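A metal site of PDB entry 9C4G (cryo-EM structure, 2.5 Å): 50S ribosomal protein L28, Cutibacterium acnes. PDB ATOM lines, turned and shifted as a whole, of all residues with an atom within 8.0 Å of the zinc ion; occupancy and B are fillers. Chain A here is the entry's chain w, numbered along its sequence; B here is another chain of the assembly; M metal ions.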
ATOM      1  N   VAL A   4       3.659  16.773 -23.032  1.00  0.00           N
ATOM      2  CA  VAL A   4       4.845  16.691 -22.195  1.00  0.00           C
ATOM      3  C   VAL A   4       5.646  17.973 -22.380  1.00  0.00           C
ATOM      4  O   VAL A   4       5.961  18.347 -23.522  1.00  0.00           O
ATOM      5  CB  VAL A   4       5.707  15.460 -22.516  1.00  0.00           C
ATOM      6  CG1 VAL A   4       6.732  15.252 -21.422  1.00  0.00           C
ATOM      7  CG2 VAL A   4       4.830  14.223 -22.673  1.00  0.00           C
ATOM      8  N   CYS A   5       5.975  18.631 -21.273  1.00  0.00           N
ATOM      9  CA  CYS A   5       6.742  19.861 -21.323  1.00  0.00           C
ATOM     10  C   CYS A   5       8.225  19.550 -21.481  1.00  0.00           C
ATOM     11  O   CYS A   5       8.788  18.775 -20.709  1.00  0.00           O
ATOM     12  CB  CYS A   5       6.511  20.680 -20.054  1.00  0.00           C
ATOM     13  SG  CYS A   5       7.377  22.270 -20.007  1.00  0.00           S
ATOM     14  N   ASP A   6       8.853  20.145 -22.494  1.00  0.00           N
ATOM     15  CA  ASP A   6      10.283  19.963 -22.690  1.00  0.00           C
ATOM     16  C   ASP A   6      11.109  20.609 -21.582  1.00  0.00           C
ATOM     17  O   ASP A   6      12.279  20.285 -21.427  1.00  0.00           O
ATOM     18  CB  ASP A   6      10.716  20.530 -24.047  1.00  0.00           C
ATOM     19  CG  ASP A   6      10.162  19.727 -25.203  1.00  0.00           C
ATOM     20  OD1 ASP A   6       9.676  18.591 -24.971  1.00  0.00           O
ATOM     21  OD2 ASP A   6      10.209  20.219 -26.358  1.00  0.00           O
ATOM     22  N   ILE A   7      10.508  21.520 -20.809  1.00  0.00           N
ATOM     23  CA  ILE A   7      11.088  22.049 -19.587  1.00  0.00           C
ATOM     24  C   ILE A   7      10.239  21.574 -18.422  1.00  0.00           C
ATOM     25  O   ILE A   7       9.021  21.789 -18.406  1.00  0.00           O
ATOM     26  CB  ILE A   7      11.173  23.587 -19.621  1.00  0.00           C
ATOM     27  CG1 ILE A   7      12.241  24.054 -20.599  1.00  0.00           C
ATOM     28  CG2 ILE A   7      11.427  24.145 -18.230  1.00  0.00           C
ATOM     29  CD1 ILE A   7      11.697  24.890 -21.721  1.00  0.00           C
ATOM     30  N   CYS A   8      10.874  20.950 -17.441  1.00  0.00           N
ATOM     31  CA  CYS A   8      10.285  20.453 -16.202  1.00  0.00           C
ATOM     32  C   CYS A   8       9.586  19.108 -16.382  1.00  0.00           C
ATOM     33  O   CYS A   8       9.126  18.539 -15.388  1.00  0.00           O
ATOM     34  CB  CYS A   8       9.286  21.444 -15.567  1.00  0.00           C
ATOM     35  SG  CYS A   8       7.596  21.350 -16.220  1.00  0.00           S
ATOM     36  N   ALA A   9       9.493  18.564 -17.599  1.00  0.00           N
ATOM     37  CA  ALA A   9       9.026  17.197 -17.833  1.00  0.00           C
ATOM     38  C   ALA A   9       7.634  16.938 -17.262  1.00  0.00           C
ATOM     39  O   ALA A   9       7.361  15.872 -16.719  1.00  0.00           O
ATOM     40  CB  ALA A   9      10.034  16.171 -17.295  1.00  0.00           C
ATOM     41  N   LYS A  10       6.746  17.918 -17.391  1.00  0.00           N
ATOM     42  CA  LYS A  10       5.387  17.753 -16.912  1.00  0.00           C
ATOM     43  C   LYS A  10       4.605  16.853 -17.861  1.00  0.00           C
ATOM     44  O   LYS A  10       4.638  17.032 -19.077  1.00  0.00           O
ATOM     45  CB  LYS A  10       4.704  19.118 -16.784  1.00  0.00           C
ATOM     46  CG  LYS A  10       3.595  19.141 -15.760  1.00  0.00           C
ATOM     47  CD  LYS A  10       2.585  20.240 -16.050  1.00  0.00           C
ATOM     48  CE  LYS A  10       3.101  21.601 -15.628  1.00  0.00           C
ATOM     49  NZ  LYS A  10       2.648  21.938 -14.258  1.00  0.00           N
ATOM     50  N   ARG A  11       3.890  15.884 -17.303  1.00  0.00           N
ATOM     51  CA  ARG A  11       3.234  14.821 -18.060  1.00  0.00           C
ATOM     52  C   ARG A  11       1.785  14.686 -17.610  1.00  0.00           C
ATOM     53  O   ARG A  11       1.413  15.162 -16.537  1.00  0.00           O
ATOM     54  CB  ARG A  11       3.978  13.490 -17.881  1.00  0.00           C
ATOM     55  CG  ARG A  11       3.978  12.943 -16.471  1.00  0.00           C
ATOM     56  CD  ARG A  11       4.977  11.821 -16.331  1.00  0.00           C
ATOM     57  NE  ARG A  11       4.622  10.668 -17.155  1.00  0.00           N
ATOM     58  CZ  ARG A  11       5.482   9.765 -17.604  1.00  0.00           C
ATOM     59  NH1 ARG A  11       6.772   9.856 -17.326  1.00  0.00           N
ATOM     60  NH2 ARG A  11       5.041   8.753 -18.339  1.00  0.00           N
ATOM     61  N   PRO A  31      -1.299  18.525 -19.418  1.00  0.00           N
ATOM     62  CA  PRO A  31      -0.797  19.876 -19.145  1.00  0.00           C
ATOM     63  C   PRO A  31      -1.068  20.803 -20.315  1.00  0.00           C
ATOM     64  O   PRO A  31      -1.186  20.374 -21.472  1.00  0.00           O
ATOM     65  CB  PRO A  31       0.701  19.672 -18.933  1.00  0.00           C
ATOM     66  CG  PRO A  31       1.015  18.394 -19.580  1.00  0.00           C
ATOM     67  CD  PRO A  31      -0.203  17.542 -19.520  1.00  0.00           C
ATOM     68  N   ASN A  32      -1.187  22.090 -20.012  1.00  0.00           N
ATOM     69  CA  ASN A  32      -1.492  23.094 -21.021  1.00  0.00           C
ATOM     70  C   ASN A  32      -0.202  23.404 -21.774  1.00  0.00           C
ATOM     71  O   ASN A  32       0.517  24.371 -21.504  1.00  0.00           O
ATOM     72  CB  ASN A  32      -2.099  24.339 -20.383  1.00  0.00           C
ATOM     73  CG  ASN A  32      -2.538  25.369 -21.393  1.00  0.00           C
ATOM     74  OD1 ASN A  32      -2.743  25.058 -22.571  1.00  0.00           O
ATOM     75  ND2 ASN A  32      -2.649  26.614 -20.958  1.00  0.00           N
ATOM     76  N   ILE A  33       0.113  22.530 -22.735  1.00  0.00           N
ATOM     77  CA  ILE A  33       1.351  22.617 -23.505  1.00  0.00           C
ATOM     78  C   ILE A  33       1.137  23.523 -24.709  1.00  0.00           C
ATOM     79  O   ILE A  33       0.186  23.337 -25.471  1.00  0.00           O
ATOM     80  CB  ILE A  33       1.810  21.216 -23.948  1.00  0.00           C
ATOM     81  CG1 ILE A  33       2.213  20.371 -22.743  1.00  0.00           C
ATOM     82  CG2 ILE A  33       2.965  21.310 -24.930  1.00  0.00           C
ATOM     83  CD1 ILE A  33       3.306  20.973 -21.908  1.00  0.00           C
ATOM     84  N   ASN A  48       7.896  22.629 -26.930  1.00  0.00           N
ATOM     85  CA  ASN A  48       6.604  22.355 -26.303  1.00  0.00           C
ATOM     86  C   ASN A  48       6.767  22.586 -24.811  1.00  0.00           C
ATOM     87  O   ASN A  48       7.326  21.748 -24.104  1.00  0.00           O
ATOM     88  CB  ASN A  48       6.151  20.929 -26.610  1.00  0.00           C
ATOM     89  CG  ASN A  48       5.681  20.751 -28.023  1.00  0.00           C
ATOM     90  OD1 ASN A  48       5.041  21.627 -28.593  1.00  0.00           O
ATOM     91  ND2 ASN A  48       6.000  19.608 -28.609  1.00  0.00           N
ATOM     92  N   VAL A  49       6.286  23.717 -24.328  1.00  0.00           N
ATOM     93  CA  VAL A  49       6.468  24.112 -22.940  1.00  0.00           C
ATOM     94  C   VAL A  49       5.104  24.329 -22.308  1.00  0.00           C
ATOM     95  O   VAL A  49       4.142  24.703 -22.971  1.00  0.00           O
ATOM     96  CB  VAL A  49       7.344  25.380 -22.816  1.00  0.00           C
ATOM     97  CG1 VAL A  49       8.617  25.230 -23.621  1.00  0.00           C
ATOM     98  CG2 VAL A  49       6.582  26.607 -23.278  1.00  0.00           C
ATOM     99  N   CYS A  50       5.021  24.075 -21.001  1.00  0.00           N
ATOM    100  CA  CYS A  50       3.766  24.315 -20.296  1.00  0.00           C
ATOM    101  C   CYS A  50       3.608  25.795 -19.969  1.00  0.00           C
ATOM    102  O   CYS A  50       4.569  26.566 -19.966  1.00  0.00           O
ATOM    103  CB  CYS A  50       3.700  23.476 -19.018  1.00  0.00           C
ATOM    104  SG  CYS A  50       4.928  23.919 -17.760  1.00  0.00           S
ATOM    105  N   THR A  51       2.360  26.185 -19.706  1.00  0.00           N
ATOM    106  CA  THR A  51       2.104  27.566 -19.328  1.00  0.00           C
ATOM    107  C   THR A  51       2.660  27.914 -17.950  1.00  0.00           C
ATOM    108  O   THR A  51       2.840  29.099 -17.657  1.00  0.00           O
ATOM    109  CB  THR A  51       0.602  27.854 -19.362  1.00  0.00           C
ATOM    110  OG1 THR A  51      -0.113  26.781 -18.767  1.00  0.00           O
ATOM    111  CG2 THR A  51       0.129  28.047 -20.787  1.00  0.00           C
ATOM    112  N   SER A  52       2.945  26.915 -17.119  1.00  0.00           N
ATOM    113  CA  SER A  52       3.572  27.190 -15.826  1.00  0.00           C
ATOM    114  C   SER A  52       5.028  27.609 -15.990  1.00  0.00           C
ATOM    115  O   SER A  52       5.515  28.457 -15.251  1.00  0.00           O
ATOM    116  CB  SER A  52       3.458  25.967 -14.927  1.00  0.00           C
ATOM    117  OG  SER A  52       2.114  25.677 -14.627  1.00  0.00           O
ATOM    118  N   CYS A  53       5.732  27.003 -16.946  1.00  0.00           N
ATOM    119  CA  CYS A  53       7.096  27.429 -17.247  1.00  0.00           C
ATOM    120  C   CYS A  53       7.123  28.673 -18.123  1.00  0.00           C
ATOM    121  O   CYS A  53       8.146  29.346 -18.190  1.00  0.00           O
ATOM    122  CB  CYS A  53       7.860  26.290 -17.927  1.00  0.00           C
ATOM    123  SG  CYS A  53       8.006  24.790 -16.931  1.00  0.00           S
ATOM    124  N   LEU A  54       6.012  28.968 -18.805  1.00  0.00           N
ATOM    125  CA  LEU A  54       5.885  30.238 -19.514  1.00  0.00           C
ATOM    126  C   LEU A  54       5.674  31.385 -18.540  1.00  0.00           C
ATOM    127  O   LEU A  54       6.263  32.454 -18.692  1.00  0.00           O
ATOM    128  CB  LEU A  54       4.730  30.140 -20.505  1.00  0.00           C
ATOM    129  CG  LEU A  54       4.844  30.635 -21.943  1.00  0.00           C
ATOM    130  CD1 LEU A  54       6.077  30.090 -22.627  1.00  0.00           C
ATOM    131  CD2 LEU A  54       3.599  30.240 -22.718  1.00  0.00           C
ATOM    132  N   ARG A  58      10.789  30.450 -17.420  1.00  0.00           N
ATOM    133  CA  ARG A  58      11.817  29.443 -17.512  1.00  0.00           C
ATOM    134  C   ARG A  58      12.258  29.165 -18.942  1.00  0.00           C
ATOM    135  O   ARG A  58      13.146  28.328 -19.157  1.00  0.00           O
ATOM    136  CB  ARG A  58      11.338  28.140 -16.866  1.00  0.00           C
ATOM    137  CG  ARG A  58      11.237  28.204 -15.349  1.00  0.00           C
ATOM    138  CD  ARG A  58      10.421  27.050 -14.796  1.00  0.00           C
ATOM    139  NE  ARG A  58      11.141  25.791 -14.837  1.00  0.00           N
ATOM    140  CZ  ARG A  58      10.851  24.732 -14.091  1.00  0.00           C
ATOM    141  NH1 ARG A  58       9.845  24.753 -13.233  1.00  0.00           N
ATOM    142  NH2 ARG A  58      11.577  23.625 -14.222  1.00  0.00           N
ATOM    143  P     C B 486      -1.106  21.922 -15.952  1.00  0.00           P
ATOM    144  OP1   C B 486      -0.390  22.347 -17.184  1.00  0.00           O
ATOM    145  OP2   C B 486      -0.453  22.100 -14.634  1.00  0.00           O
ATOM    146  O5'   C B 486      -2.495  22.706 -15.904  1.00  0.00           O
ATOM    147  C5'   C B 486      -3.387  22.670 -17.000  1.00  0.00           C
ATOM    148  C4'   C B 486      -4.655  23.402 -16.685  1.00  0.00           C
ATOM    149  O4'   C B 486      -5.342  22.744 -15.594  1.00  0.00           O
ATOM    150  C3'   C B 486      -4.482  24.821 -16.182  1.00  0.00           C
ATOM    151  O3'   C B 486      -4.248  25.746 -17.231  1.00  0.00           O
ATOM    152  C2'   C B 486      -5.775  25.063 -15.412  1.00  0.00           C
ATOM    153  O2'   C B 486      -6.843  25.336 -16.301  1.00  0.00           O
ATOM    154  C1'   C B 486      -6.003  23.697 -14.780  1.00  0.00           C
ATOM    155  N1    C B 486      -5.451  23.614 -13.415  1.00  0.00           N
ATOM    156  C2    C B 486      -6.237  24.071 -12.356  1.00  0.00           C
ATOM    157  O2    C B 486      -7.366  24.518 -12.592  1.00  0.00           O
ATOM    158  N3    C B 486      -5.745  24.016 -11.098  1.00  0.00           N
ATOM    159  C4    C B 486      -4.536  23.531 -10.882  1.00  0.00           C
ATOM    160  N4    C B 486      -4.089  23.495  -9.635  1.00  0.00           N
ATOM    161  C5    C B 486      -3.703  23.056 -11.946  1.00  0.00           C
ATOM    162  C6    C B 486      -4.209  23.121 -13.183  1.00  0.00           C
HETATM  163 ZN    ZN M   1       7.010  22.887 -17.816  1.00  0.00          ZN
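The zinc ion is bound by SG of Cys 8 (2.3 Å).
The side-chain sulfur (SG) of Cys 5 binds the zinc ion (2.3 Å).
The side-chain sulfur (SG) of Cys 53 is bound to the zinc ion (2.3 Å).
The zinc ion is bound by the side-chain sulfur (SG) of Cys 50, 2.3 Å away.
The zinc ion is bound by O of Ile 7.
Of the 20 residues printed, 5 come within 4 Å of the zinc ion.
N of Lys 10 lies close to SG of Cys 8 (3.7 Å).
O of Lys 10 sits at hydrogen-bond distance from N of Cys 5 (3.0 Å).
The backbone carbonyl oxygen of Cys 53 lies within hydrogen-bond range of the backbone NH of Arg 58 (3.0 Å).
SG of Cys 50 sits close to N of Ser 52 (3.6 Å).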
